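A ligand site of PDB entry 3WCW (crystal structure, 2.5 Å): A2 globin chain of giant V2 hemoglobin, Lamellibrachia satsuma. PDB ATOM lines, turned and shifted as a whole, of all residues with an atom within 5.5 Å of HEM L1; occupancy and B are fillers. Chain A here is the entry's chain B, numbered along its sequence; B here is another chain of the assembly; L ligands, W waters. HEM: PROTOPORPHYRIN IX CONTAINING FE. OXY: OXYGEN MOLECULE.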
ATOM      1  N   TRP A  33       0.568 -36.051  -9.540  1.00  0.00           N
ATOM      2  CA  TRP A  33       1.812 -35.319  -9.719  1.00  0.00           C
ATOM      3  C   TRP A  33       2.542 -35.506 -11.035  1.00  0.00           C
ATOM      4  O   TRP A  33       3.308 -34.627 -11.450  1.00  0.00           O
ATOM      5  CB  TRP A  33       2.748 -35.597  -8.549  1.00  0.00           C
ATOM      6  CG  TRP A  33       2.299 -34.854  -7.356  1.00  0.00           C
ATOM      7  CD1 TRP A  33       1.594 -35.344  -6.304  1.00  0.00           C
ATOM      8  CD2 TRP A  33       2.464 -33.459  -7.127  1.00  0.00           C
ATOM      9  NE1 TRP A  33       1.298 -34.325  -5.429  1.00  0.00           N
ATOM     10  CE2 TRP A  33       1.825 -33.159  -5.905  1.00  0.00           C
ATOM     11  CE3 TRP A  33       3.083 -32.428  -7.843  1.00  0.00           C
ATOM     12  CZ2 TRP A  33       1.786 -31.869  -5.375  1.00  0.00           C
ATOM     13  CZ3 TRP A  33       3.058 -31.131  -7.313  1.00  0.00           C
ATOM     14  CH2 TRP A  33       2.406 -30.870  -6.089  1.00  0.00           C
ATOM     15  N   ALA A  43       7.589 -26.159 -12.006  1.00  0.00           N
ATOM     16  CA  ALA A  43       7.120 -26.290 -10.625  1.00  0.00           C
ATOM     17  C   ALA A  43       8.022 -27.151  -9.749  1.00  0.00           C
ATOM     18  O   ALA A  43       8.034 -27.004  -8.524  1.00  0.00           O
ATOM     19  CB  ALA A  43       5.704 -26.855 -10.626  1.00  0.00           C
ATOM     20  N   MET A  46      10.496 -26.069  -6.759  1.00  0.00           N
ATOM     21  CA  MET A  46       9.989 -25.773  -5.422  1.00  0.00           C
ATOM     22  C   MET A  46      10.037 -26.957  -4.465  1.00  0.00           C
ATOM     23  O   MET A  46       9.907 -26.793  -3.254  1.00  0.00           O
ATOM     24  CB  MET A  46       8.548 -25.246  -5.505  1.00  0.00           C
ATOM     25  CG  MET A  46       8.435 -23.864  -6.124  1.00  0.00           C
ATOM     26  SD  MET A  46       6.731 -23.373  -6.402  1.00  0.00           S
ATOM     27  CE  MET A  46       6.205 -23.025  -4.709  1.00  0.00           C
ATOM     28  N   PHE A  47      10.241 -28.152  -5.019  1.00  0.00           N
ATOM     29  CA  PHE A  47      10.277 -29.354  -4.208  1.00  0.00           C
ATOM     30  C   PHE A  47      11.659 -29.989  -4.114  1.00  0.00           C
ATOM     31  O   PHE A  47      11.773 -31.199  -3.977  1.00  0.00           O
ATOM     32  CB  PHE A  47       9.301 -30.388  -4.795  1.00  0.00           C
ATOM     33  CG  PHE A  47       7.901 -29.871  -4.966  1.00  0.00           C
ATOM     34  CD1 PHE A  47       6.979 -29.965  -3.927  1.00  0.00           C
ATOM     35  CD2 PHE A  47       7.489 -29.332  -6.185  1.00  0.00           C
ATOM     36  CE1 PHE A  47       5.681 -29.533  -4.096  1.00  0.00           C
ATOM     37  CE2 PHE A  47       6.182 -28.897  -6.357  1.00  0.00           C
ATOM     38  CZ  PHE A  47       5.278 -28.997  -5.312  1.00  0.00           C
ATOM     39  N   ARG A  49      13.603 -30.193  -1.742  1.00  0.00           N
ATOM     40  CA  ARG A  49      13.844 -30.896  -0.475  1.00  0.00           C
ATOM     41  C   ARG A  49      13.255 -32.298  -0.436  1.00  0.00           C
ATOM     42  O   ARG A  49      13.749 -33.168   0.293  1.00  0.00           O
ATOM     43  CB  ARG A  49      13.267 -30.100   0.691  1.00  0.00           C
ATOM     44  CG  ARG A  49      13.693 -30.657   2.047  1.00  0.00           C
ATOM     45  CD  ARG A  49      12.986 -29.953   3.187  1.00  0.00           C
ATOM     46  NE  ARG A  49      11.599 -30.399   3.350  1.00  0.00           N
ATOM     47  CZ  ARG A  49      11.262 -31.606   3.791  1.00  0.00           C
ATOM     48  NH1 ARG A  49      12.201 -32.475   4.117  1.00  0.00           N
ATOM     49  NH2 ARG A  49       9.984 -31.936   3.925  1.00  0.00           N
ATOM     50  N   VAL A  50      12.203 -32.522  -1.212  1.00  0.00           N
ATOM     51  CA  VAL A  50      11.534 -33.812  -1.235  1.00  0.00           C
ATOM     52  C   VAL A  50      11.650 -34.490  -2.602  1.00  0.00           C
ATOM     53  O   VAL A  50      10.710 -35.127  -3.094  1.00  0.00           O
ATOM     54  CB  VAL A  50      10.041 -33.644  -0.818  1.00  0.00           C
ATOM     55  CG1 VAL A  50       9.963 -33.058   0.588  1.00  0.00           C
ATOM     56  CG2 VAL A  50       9.319 -32.726  -1.787  1.00  0.00           C
ATOM     57  N   HIS A  63       5.867 -36.935   0.385  1.00  0.00           N
ATOM     58  CA  HIS A  63       5.344 -35.593   0.156  1.00  0.00           C
ATOM     59  C   HIS A  63       3.932 -35.733  -0.409  1.00  0.00           C
ATOM     60  O   HIS A  63       2.968 -35.152   0.130  1.00  0.00           O
ATOM     61  CB  HIS A  63       6.220 -34.814  -0.830  1.00  0.00           C
ATOM     62  CG  HIS A  63       5.586 -33.544  -1.316  1.00  0.00           C
ATOM     63  ND1 HIS A  63       5.323 -32.482  -0.474  1.00  0.00           N
ATOM     64  CD2 HIS A  63       5.048 -33.219  -2.515  1.00  0.00           C
ATOM     65  CE1 HIS A  63       4.649 -31.554  -1.140  1.00  0.00           C
ATOM     66  NE2 HIS A  63       4.468 -31.976  -2.383  1.00  0.00           N
ATOM     67  N   ARG A  66       1.490 -36.462   2.090  1.00  0.00           N
ATOM     68  CA  ARG A  66       1.045 -35.360   2.937  1.00  0.00           C
ATOM     69  C   ARG A  66       0.029 -34.459   2.224  1.00  0.00           C
ATOM     70  O   ARG A  66      -0.954 -34.033   2.818  1.00  0.00           O
ATOM     71  CB  ARG A  66       2.239 -34.533   3.424  1.00  0.00           C
ATOM     72  CG  ARG A  66       3.067 -35.220   4.473  1.00  0.00           C
ATOM     73  CD  ARG A  66       4.161 -34.310   4.992  1.00  0.00           C
ATOM     74  NE  ARG A  66       5.198 -34.057   3.995  1.00  0.00           N
ATOM     75  CZ  ARG A  66       6.247 -34.840   3.810  1.00  0.00           C
ATOM     76  NH1 ARG A  66       7.136 -34.533   2.870  1.00  0.00           N
ATOM     77  NH2 ARG A  66       6.416 -35.915   4.549  1.00  0.00           N
ATOM     78  N   VAL A  67       0.273 -34.173   0.949  1.00  0.00           N
ATOM     79  CA  VAL A  67      -0.626 -33.329   0.166  1.00  0.00           C
ATOM     80  C   VAL A  67      -2.042 -33.930   0.124  1.00  0.00           C
ATOM     81  O   VAL A  67      -3.030 -33.223   0.356  1.00  0.00           O
ATOM     82  CB  VAL A  67      -0.133 -33.157  -1.302  1.00  0.00           C
ATOM     83  CG1 VAL A  67      -1.153 -32.338  -2.103  1.00  0.00           C
ATOM     84  CG2 VAL A  67       1.233 -32.487  -1.314  1.00  0.00           C
ATOM     85  N   GLY A  70      -3.761 -33.607   3.127  1.00  0.00           N
ATOM     86  CA  GLY A  70      -4.215 -32.235   3.261  1.00  0.00           C
ATOM     87  C   GLY A  70      -5.601 -32.084   2.657  1.00  0.00           C
ATOM     88  O   GLY A  70      -6.494 -31.543   3.296  1.00  0.00           O
ATOM     89  N   LEU A  71      -5.766 -32.553   1.423  1.00  0.00           N
ATOM     90  CA  LEU A  71      -7.053 -32.484   0.754  1.00  0.00           C
ATOM     91  C   LEU A  71      -8.098 -33.271   1.539  1.00  0.00           C
ATOM     92  O   LEU A  71      -9.208 -32.807   1.737  1.00  0.00           O
ATOM     93  CB  LEU A  71      -6.967 -33.055  -0.667  1.00  0.00           C
ATOM     94  CG  LEU A  71      -6.398 -32.201  -1.796  1.00  0.00           C
ATOM     95  CD1 LEU A  71      -6.187 -33.088  -3.031  1.00  0.00           C
ATOM     96  CD2 LEU A  71      -7.348 -31.041  -2.101  1.00  0.00           C
ATOM     97  N   CYS A  74      -9.433 -31.286   4.401  1.00  0.00           N
ATOM     98  CA  CYS A  74     -10.327 -30.222   3.967  1.00  0.00           C
ATOM     99  C   CYS A  74     -11.660 -30.772   3.477  1.00  0.00           C
ATOM    100  O   CYS A  74     -12.726 -30.298   3.903  1.00  0.00           O
ATOM    101  CB  CYS A  74      -9.706 -29.394   2.854  1.00  0.00           C
ATOM    102  SG  CYS A  74      -8.188 -28.554   3.358  1.00  0.00           S
ATOM    103  N   LEU A  91      -2.783 -24.848   6.492  1.00  0.00           N
ATOM    104  CA  LEU A  91      -2.180 -25.145   5.200  1.00  0.00           C
ATOM    105  C   LEU A  91      -1.641 -23.850   4.581  1.00  0.00           C
ATOM    106  O   LEU A  91      -0.593 -23.855   3.949  1.00  0.00           O
ATOM    107  CB  LEU A  91      -3.206 -25.786   4.269  1.00  0.00           C
ATOM    108  CG  LEU A  91      -3.756 -27.158   4.667  1.00  0.00           C
ATOM    109  CD1 LEU A  91      -4.879 -27.561   3.733  1.00  0.00           C
ATOM    110  CD2 LEU A  91      -2.647 -28.202   4.650  1.00  0.00           C
ATOM    111  N   GLN A  94       1.774 -23.240   6.000  1.00  0.00           N
ATOM    112  CA  GLN A  94       2.742 -24.180   5.465  1.00  0.00           C
ATOM    113  C   GLN A  94       3.218 -23.800   4.068  1.00  0.00           C
ATOM    114  O   GLN A  94       4.244 -24.290   3.611  1.00  0.00           O
ATOM    115  CB  GLN A  94       2.154 -25.600   5.522  1.00  0.00           C
ATOM    116  CG  GLN A  94       1.719 -26.000   6.942  1.00  0.00           C
ATOM    117  CD  GLN A  94       1.009 -27.357   7.046  1.00  0.00           C
ATOM    118  OE1 GLN A  94      -0.022 -27.582   6.401  1.00  0.00           O
ATOM    119  NE2 GLN A  94       1.565 -28.252   7.845  1.00  0.00           N
ATOM    120  N   HIS A  95       2.477 -22.915   3.398  1.00  0.00           N
ATOM    121  CA  HIS A  95       2.816 -22.454   2.050  1.00  0.00           C
ATOM    122  C   HIS A  95       3.186 -20.973   1.952  1.00  0.00           C
ATOM    123  O   HIS A  95       3.979 -20.587   1.110  1.00  0.00           O
ATOM    124  CB  HIS A  95       1.658 -22.687   1.080  1.00  0.00           C
ATOM    125  CG  HIS A  95       1.352 -24.134   0.830  1.00  0.00           C
ATOM    126  ND1 HIS A  95       0.747 -24.945   1.767  1.00  0.00           N
ATOM    127  CD2 HIS A  95       1.550 -24.915  -0.263  1.00  0.00           C
ATOM    128  CE1 HIS A  95       0.581 -26.147   1.263  1.00  0.00           C
ATOM    129  NE2 HIS A  95       1.062 -26.160   0.044  1.00  0.00           N
ATOM    130  N   ARG A  98       6.378 -19.837   0.326  1.00  0.00           N
ATOM    131  CA  ARG A  98       6.882 -20.510  -0.863  1.00  0.00           C
ATOM    132  C   ARG A  98       6.594 -19.900  -2.231  1.00  0.00           C
ATOM    133  O   ARG A  98       7.063 -20.402  -3.240  1.00  0.00           O
ATOM    134  CB  ARG A  98       6.421 -21.969  -0.807  1.00  0.00           C
ATOM    135  CG  ARG A  98       6.834 -22.633   0.511  1.00  0.00           C
ATOM    136  CD  ARG A  98       6.299 -24.042   0.668  1.00  0.00           C
ATOM    137  NE  ARG A  98       6.689 -24.644   1.939  1.00  0.00           N
ATOM    138  CZ  ARG A  98       7.928 -25.004   2.267  1.00  0.00           C
ATOM    139  NH1 ARG A  98       8.175 -25.544   3.454  1.00  0.00           N
ATOM    140  NH2 ARG A  98       8.925 -24.838   1.405  1.00  0.00           N
ATOM    141  N   VAL A 100       3.655 -19.539  -4.170  1.00  0.00           N
ATOM    142  CA  VAL A 100       2.821 -20.353  -5.054  1.00  0.00           C
ATOM    143  C   VAL A 100       1.873 -19.456  -5.874  1.00  0.00           C
ATOM    144  O   VAL A 100       1.025 -18.769  -5.316  1.00  0.00           O
ATOM    145  CB  VAL A 100       1.995 -21.368  -4.222  1.00  0.00           C
ATOM    146  CG1 VAL A 100       1.230 -22.295  -5.132  1.00  0.00           C
ATOM    147  CG2 VAL A 100       2.919 -22.154  -3.296  1.00  0.00           C
ATOM    148  N   GLN A 104      -0.360 -22.061 -10.592  1.00  0.00           N
ATOM    149  CA  GLN A 104       0.062 -23.365 -10.121  1.00  0.00           C
ATOM    150  C   GLN A 104      -1.072 -24.010  -9.315  1.00  0.00           C
ATOM    151  O   GLN A 104      -1.367 -25.195  -9.499  1.00  0.00           O
ATOM    152  CB  GLN A 104       1.327 -23.222  -9.266  1.00  0.00           C
ATOM    153  CG  GLN A 104       2.483 -22.550  -9.993  1.00  0.00           C
ATOM    154  CD  GLN A 104       3.749 -22.443  -9.145  1.00  0.00           C
ATOM    155  OE1 GLN A 104       3.743 -21.870  -8.047  1.00  0.00           O
ATOM    156  NE2 GLN A 104       4.856 -22.993  -9.656  1.00  0.00           N
ATOM    157  N   TYR A 105      -1.714 -23.236  -8.439  1.00  0.00           N
ATOM    158  CA  TYR A 105      -2.812 -23.776  -7.646  1.00  0.00           C
ATOM    159  C   TYR A 105      -3.857 -24.331  -8.611  1.00  0.00           C
ATOM    160  O   TYR A 105      -4.457 -25.376  -8.339  1.00  0.00           O
ATOM    161  CB  TYR A 105      -3.450 -22.693  -6.743  1.00  0.00           C
ATOM    162  CG  TYR A 105      -2.768 -22.481  -5.400  1.00  0.00           C
ATOM    163  CD1 TYR A 105      -2.745 -23.492  -4.424  1.00  0.00           C
ATOM    164  CD2 TYR A 105      -2.130 -21.269  -5.095  1.00  0.00           C
ATOM    165  CE1 TYR A 105      -2.095 -23.306  -3.204  1.00  0.00           C
ATOM    166  CE2 TYR A 105      -1.486 -21.071  -3.880  1.00  0.00           C
ATOM    167  CZ  TYR A 105      -1.468 -22.089  -2.935  1.00  0.00           C
ATOM    168  OH  TYR A 105      -0.796 -21.886  -1.739  1.00  0.00           O
ATOM    169  N   VAL A 108      -2.559 -27.709 -10.043  1.00  0.00           N
ATOM    170  CA  VAL A 108      -2.702 -28.785  -9.088  1.00  0.00           C
ATOM    171  C   VAL A 108      -4.185 -29.125  -8.923  1.00  0.00           C
ATOM    172  O   VAL A 108      -4.542 -30.269  -8.626  1.00  0.00           O
ATOM    173  CB  VAL A 108      -2.045 -28.389  -7.761  1.00  0.00           C
ATOM    174  CG1 VAL A 108      -2.363 -29.414  -6.686  1.00  0.00           C
ATOM    175  CG2 VAL A 108      -0.546 -28.267  -7.962  1.00  0.00           C
ATOM    176  N   VAL A 112      -5.587 -32.854  -9.639  1.00  0.00           N
ATOM    177  CA  VAL A 112      -6.448 -33.534  -8.677  1.00  0.00           C
ATOM    178  C   VAL A 112      -7.778 -33.969  -9.295  1.00  0.00           C
ATOM    179  O   VAL A 112      -8.254 -35.078  -9.037  1.00  0.00           O
ATOM    180  CB  VAL A 112      -6.714 -32.630  -7.456  1.00  0.00           C
ATOM    181  CG1 VAL A 112      -7.796 -33.247  -6.567  1.00  0.00           C
ATOM    182  CG2 VAL A 112      -5.416 -32.429  -6.660  1.00  0.00           C
ATOM    183  N   ILE A 137     -11.235 -24.396  -1.513  1.00  0.00           N
ATOM    184  CA  ILE A 137     -10.101 -24.912  -0.744  1.00  0.00           C
ATOM    185  C   ILE A 137      -8.778 -24.209  -1.063  1.00  0.00           C
ATOM    186  O   ILE A 137      -8.005 -23.913  -0.157  1.00  0.00           O
ATOM    187  CB  ILE A 137      -9.937 -26.438  -0.946  1.00  0.00           C
ATOM    188  CG1 ILE A 137     -11.201 -27.151  -0.443  1.00  0.00           C
ATOM    189  CG2 ILE A 137      -8.700 -26.942  -0.189  1.00  0.00           C
ATOM    190  CD1 ILE A 137     -11.142 -28.673  -0.478  1.00  0.00           C
ATOM    191  N   THR A 138      -8.524 -23.963  -2.344  1.00  0.00           N
ATOM    192  CA  THR A 138      -7.298 -23.279  -2.733  1.00  0.00           C
ATOM    193  C   THR A 138      -7.338 -21.853  -2.199  1.00  0.00           C
ATOM    194  O   THR A 138      -6.360 -21.371  -1.624  1.00  0.00           O
ATOM    195  CB  THR A 138      -7.086 -23.246  -4.284  1.00  0.00           C
ATOM    196  OG1 THR A 138      -8.334 -22.994  -4.928  1.00  0.00           O
ATOM    197  CG2 THR A 138      -6.536 -24.575  -4.797  1.00  0.00           C
ATOM    198  N   ILE A 141      -6.177 -21.670   1.172  1.00  0.00           N
ATOM    199  CA  ILE A 141      -4.731 -21.877   1.247  1.00  0.00           C
ATOM    200  C   ILE A 141      -3.930 -20.618   0.912  1.00  0.00           C
ATOM    201  O   ILE A 141      -2.837 -20.415   1.454  1.00  0.00           O
ATOM    202  CB  ILE A 141      -4.251 -22.982   0.256  1.00  0.00           C
ATOM    203  CG1 ILE A 141      -5.116 -24.239   0.377  1.00  0.00           C
ATOM    204  CG2 ILE A 141      -2.783 -23.301   0.535  1.00  0.00           C
ATOM    205  CD1 ILE A 141      -4.704 -25.187   1.467  1.00  0.00           C
ATOM    206  N   HIS B  94       9.733 -36.982   8.590  1.00  0.00           N
ATOM    207  CA  HIS B  94       9.107 -35.676   8.510  1.00  0.00           C
ATOM    208  C   HIS B  94       8.278 -35.402   9.771  1.00  0.00           C
ATOM    209  O   HIS B  94       8.173 -34.260  10.207  1.00  0.00           O
ATOM    210  CB  HIS B  94       8.207 -35.597   7.289  1.00  0.00           C
ATOM    211  CG  HIS B  94       7.626 -34.234   7.055  1.00  0.00           C
ATOM    212  ND1 HIS B  94       8.355 -33.204   6.505  1.00  0.00           N
ATOM    213  CD2 HIS B  94       6.385 -33.735   7.308  1.00  0.00           C
ATOM    214  CE1 HIS B  94       7.582 -32.134   6.417  1.00  0.00           C
ATOM    215  NE2 HIS B  94       6.389 -32.434   6.896  1.00  0.00           N
ATOM    216  N   GLN B  98       8.959 -32.599  13.008  1.00  0.00           N
ATOM    217  CA  GLN B  98       7.819 -31.771  13.401  1.00  0.00           C
ATOM    218  C   GLN B  98       7.646 -31.805  14.925  1.00  0.00           C
ATOM    219  O   GLN B  98       7.134 -30.850  15.505  1.00  0.00           O
ATOM    220  CB  GLN B  98       6.529 -32.244  12.748  1.00  0.00           C
ATOM    221  CG  GLN B  98       6.418 -31.955  11.254  1.00  0.00           C
ATOM    222  CD  GLN B  98       5.030 -32.209  10.712  1.00  0.00           C
ATOM    223  OE1 GLN B  98       4.419 -33.228  11.017  1.00  0.00           O
ATOM    224  NE2 GLN B  98       4.536 -31.297   9.904  1.00  0.00           N
HETATM  225  CHA HEM L   1       3.911 -28.753   1.255  1.00  0.00           C
HETATM  226  CHB HEM L   1      -0.757 -29.420   1.043  1.00  0.00           C
HETATM  227  CHC HEM L   1      -0.951 -27.131  -3.194  1.00  0.00           C
HETATM  228  CHD HEM L   1       3.818 -26.509  -2.963  1.00  0.00           C
HETATM  229  C1A HEM L   1       2.654 -29.144   1.576  1.00  0.00           C
HETATM  230  C2A HEM L   1       2.346 -29.851   2.750  1.00  0.00           C
HETATM  231  C3A HEM L   1       1.024 -30.053   2.703  1.00  0.00           C
HETATM  232  C4A HEM L   1       0.500 -29.460   1.482  1.00  0.00           C
HETATM  233  CMA HEM L   1       0.155 -30.793   3.750  1.00  0.00           C
HETATM  234  CAA HEM L   1       3.304 -30.298   3.835  1.00  0.00           C
HETATM  235  CBA HEM L   1       3.577 -29.213   4.847  1.00  0.00           C
HETATM  236  CGA HEM L   1       4.551 -29.642   5.939  1.00  0.00           C
HETATM  237  O1A HEM L   1       4.190 -30.515   6.769  1.00  0.00           O
HETATM  238  O2A HEM L   1       5.645 -29.141   5.942  1.00  0.00           O
HETATM  239  C1B HEM L   1      -1.255 -28.846  -0.136  1.00  0.00           C
HETATM  240  C2B HEM L   1      -2.658 -28.872  -0.505  1.00  0.00           C
HETATM  241  C3B HEM L   1      -2.708 -28.175  -1.766  1.00  0.00           C
HETATM  242  C4B HEM L   1      -1.363 -27.818  -2.052  1.00  0.00           C
HETATM  243  CMB HEM L   1      -3.772 -29.479   0.268  1.00  0.00           C
HETATM  244  CAB HEM L   1      -3.929 -27.972  -2.496  1.00  0.00           C
HETATM  245  CBB HEM L   1      -4.248 -28.617  -3.590  1.00  0.00           C
HETATM  246  C1C HEM L   1       0.346 -26.772  -3.497  1.00  0.00           C
HETATM  247  C2C HEM L   1       0.701 -26.072  -4.738  1.00  0.00           C
HETATM  248  C3C HEM L   1       2.094 -25.871  -4.714  1.00  0.00           C
HETATM  249  C4C HEM L   1       2.523 -26.486  -3.400  1.00  0.00           C
HETATM  250  CMC HEM L   1      -0.280 -25.643  -5.842  1.00  0.00           C
HETATM  251  CAC HEM L   1       2.860 -25.271  -5.659  1.00  0.00           C
HETATM  252  CBC HEM L   1       3.240 -25.502  -6.876  1.00  0.00           C
HETATM  253  C1D HEM L   1       4.267 -27.061  -1.777  1.00  0.00           C
HETATM  254  C2D HEM L   1       5.717 -27.062  -1.327  1.00  0.00           C
HETATM  255  C3D HEM L   1       5.705 -27.698  -0.129  1.00  0.00           C
HETATM  256  C4D HEM L   1       4.309 -28.082   0.149  1.00  0.00           C
HETATM  257  CMD HEM L   1       6.871 -26.458  -2.094  1.00  0.00           C
HETATM  258  CAD HEM L   1       6.881 -27.975   0.772  1.00  0.00           C
HETATM  259  CBD HEM L   1       7.412 -29.362   0.654  1.00  0.00           C
HETATM  260  CGD HEM L   1       8.539 -29.585   1.561  1.00  0.00           C
HETATM  261  O1D HEM L   1       8.333 -30.078   2.724  1.00  0.00           O
HETATM  262  O2D HEM L   1       9.687 -29.281   1.183  1.00  0.00           O
HETATM  263  NA  HEM L   1       1.541 -28.893   0.778  1.00  0.00           N
HETATM  264  NB  HEM L   1      -0.472 -28.227  -1.032  1.00  0.00           N
HETATM  265  NC  HEM L   1       1.472 -27.004  -2.727  1.00  0.00           N
HETATM  266  ND  HEM L   1       3.482 -27.674  -0.862  1.00  0.00           N
HETATM  267 FE   HEM L   1       1.508 -27.942  -0.971  1.00  0.00          FE
HETATM  268  O1  OXY L   2       1.935 -29.441  -1.856  1.00  0.00           O
HETATM  269  O2  OXY L   2       2.671 -29.789  -2.791  1.00  0.00           O
HETATM  270  CHA HEM L   3       1.826 -31.751  16.099  1.00  0.00           C
HETATM  271  CHB HEM L   3       0.843 -36.187  14.796  1.00  0.00           C
HETATM  272  CHC HEM L   3       1.965 -37.776  19.210  1.00  0.00           C
HETATM  273  CHD HEM L   3       3.002 -33.276  20.465  1.00  0.00           C
HETATM  274  C1A HEM L   3       1.457 -32.811  15.334  1.00  0.00           C
HETATM  275  C2A HEM L   3       1.046 -32.699  14.004  1.00  0.00           C
HETATM  276  C3A HEM L   3       0.771 -33.960  13.604  1.00  0.00           C
HETATM  277  C4A HEM L   3       1.012 -34.874  14.734  1.00  0.00           C
HETATM  278  CMA HEM L   3       0.269 -34.425  12.216  1.00  0.00           C
HETATM  279  CAA HEM L   3       0.932 -31.417  13.174  1.00  0.00           C
HETATM  280  CBA HEM L   3       2.186 -31.052  12.444  1.00  0.00           C
HETATM  281  CGA HEM L   3       2.074 -29.757  11.621  1.00  0.00           C
HETATM  282  O1A HEM L   3       1.210 -29.661  10.710  1.00  0.00           O
HETATM  283  O2A HEM L   3       2.822 -28.863  11.907  1.00  0.00           O
HETATM  284  C1B HEM L   3       1.051 -37.066  15.887  1.00  0.00           C
HETATM  285  C2B HEM L   3       0.816 -38.499  15.845  1.00  0.00           C
HETATM  286  C3B HEM L   3       1.154 -38.951  17.173  1.00  0.00           C
HETATM  287  C4B HEM L   3       1.558 -37.788  17.883  1.00  0.00           C
HETATM  288  CMB HEM L   3       0.333 -39.283  14.674  1.00  0.00           C
HETATM  289  CAB HEM L   3       1.055 -40.333  17.602  1.00  0.00           C
HETATM  290  CBB HEM L   3       1.944 -41.266  17.311  1.00  0.00           C
HETATM  291  C1C HEM L   3       2.359 -36.673  19.931  1.00  0.00           C
HETATM  292  C2C HEM L   3       2.779 -36.763  21.340  1.00  0.00           C
HETATM  293  C3C HEM L   3       3.090 -35.444  21.755  1.00  0.00           C
HETATM  294  C4C HEM L   3       2.830 -34.617  20.505  1.00  0.00           C
HETATM  295  CMC HEM L   3       2.839 -38.049  22.164  1.00  0.00           C
HETATM  296  CAC HEM L   3       3.522 -35.010  22.995  1.00  0.00           C
HETATM  297  CBC HEM L   3       3.796 -35.456  24.194  1.00  0.00           C
HETATM  298  C1D HEM L   3       2.765 -32.451  19.379  1.00  0.00           C
HETATM  299  C2D HEM L   3       2.951 -30.950  19.400  1.00  0.00           C
HETATM  300  C3D HEM L   3       2.599 -30.561  18.137  1.00  0.00           C
HETATM  301  C4D HEM L   3       2.226 -31.758  17.389  1.00  0.00           C
HETATM  302  CMD HEM L   3       3.424 -30.140  20.604  1.00  0.00           C
HETATM  303  CAD HEM L   3       2.556 -29.155  17.572  1.00  0.00           C
HETATM  304  CBD HEM L   3       1.147 -28.644  17.692  1.00  0.00           C
HETATM  305  CGD HEM L   3       0.946 -27.319  17.136  1.00  0.00           C
HETATM  306  O1D HEM L   3       1.321 -26.297  17.787  1.00  0.00           O
HETATM  307  O2D HEM L   3       0.415 -27.216  16.019  1.00  0.00           O
HETATM  308  NA  HEM L   3       1.443 -34.137  15.797  1.00  0.00           N
HETATM  309  NB  HEM L   3       1.478 -36.626  17.070  1.00  0.00           N
HETATM  310  NC  HEM L   3       2.408 -35.371  19.470  1.00  0.00           N
HETATM  311  ND  HEM L   3       2.342 -32.869  18.167  1.00  0.00           N
HETATM  312 FE   HEM L   3       1.939 -34.751  17.624  1.00  0.00          FE
HETATM  313  O   HOH W   1      11.089 -28.551  -1.293  1.00  0.00           O
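Water W1 lies within hydrogen-bond range of O of Met 46 (2.9 Å), O2D of HEM L1 (2.9 Å) and N of Arg 49 (3.0 Å).
Met 46 touches HEM L1.
Phe 47 touches HEM L1.
Val 50 touches HEM L1.
His 63 touches HEM L1 (CE1 to C4D, 3.7 Å).
Arg 66 touches HEM L1 (O to CMA, 3.5 Å).
Val 67 touches HEM L1 (O to CMB, 3.8 Å).
Gly 70 touches HEM L1.
Leu 71 touches HEM L1 (N to CMB, 3.8 Å).
Leu 91 touches HEM L1 (CD2 to CMA, 3.9 Å).
Gln 94 of chain A touches HEM L1 (NE2 to O1A, 3.6 Å).
CZ of Arg 98 of chain A touches CAD of HEM L1, 3.5 Å away.
Val 100 touches HEM L1 (CG1 to CAC, 3.4 Å).
Gln 104 touches HEM L1.
Tyr 105 touches HEM L1.
Val 108 touches HEM L1.
19 residues have an atom within 4 Å of HEM L1: Met 46, Phe 47, Arg 49, Val 50, His 63, Arg 66, Val 67, Gly 70, Leu 71, Leu 91, Gln 94 of chain A, His 95, Arg 98 of chain A, Val 100, Gln 104, Tyr 105, Val 108, His 94 of chain B and Gln 98 of chain B.
The nearest printed residue that does not touch HEM L1 is Ile 141 (4.6 Å).
O of Leu 91 lies within hydrogen-bond range of ND1 of His 95 (2.8 Å).
ND1 of His 94 of chain B sits at hydrogen-bond distance from NH2 of Arg 49, 3.3 Å away.
The side-chain sulfur of Met 46 sits close to the side-chain amide oxygen of Gln 104.
The guanidinium group (NE) of Arg 98 of chain A lies within hydrogen-bond range of the backbone carbonyl oxygen (O) of Gln 94 of chain A (3.0 Å).
The side-chain sulfur (SG) of Cys 74 is in hydrogen-bond range of the backbone carbonyl oxygen (O) of Gly 70 (3.4 Å).
An iron atom (FE) of HEM L1 is bound by a ring nitrogen (NE2) of His 95, at 2.1 Å.
The guanidinium group (NH2) of Arg 49 lies within salt-bridge range of an oxygen (O1D) of HEM L1.
An oxygen (O1A) of HEM L1 is in hydrogen-bond range of a ring nitrogen (NE2) of His 94 of chain B.
O1A of HEM L1 is in hydrogen-bond range of NE2 of Gln 98 of chain B, 3.2 Å away.
A ring nitrogen (NE2) of His 63 is in hydrogen-bond range of an oxygen (O2) of OXY L2 (2.9 Å).
NE2 of Gln 94 of chain A is in hydrogen-bond range of O1A of HEM L3, 3.2 Å away.
FE of HEM L1 is bound by O1 of OXY L2 (1.8 Å).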
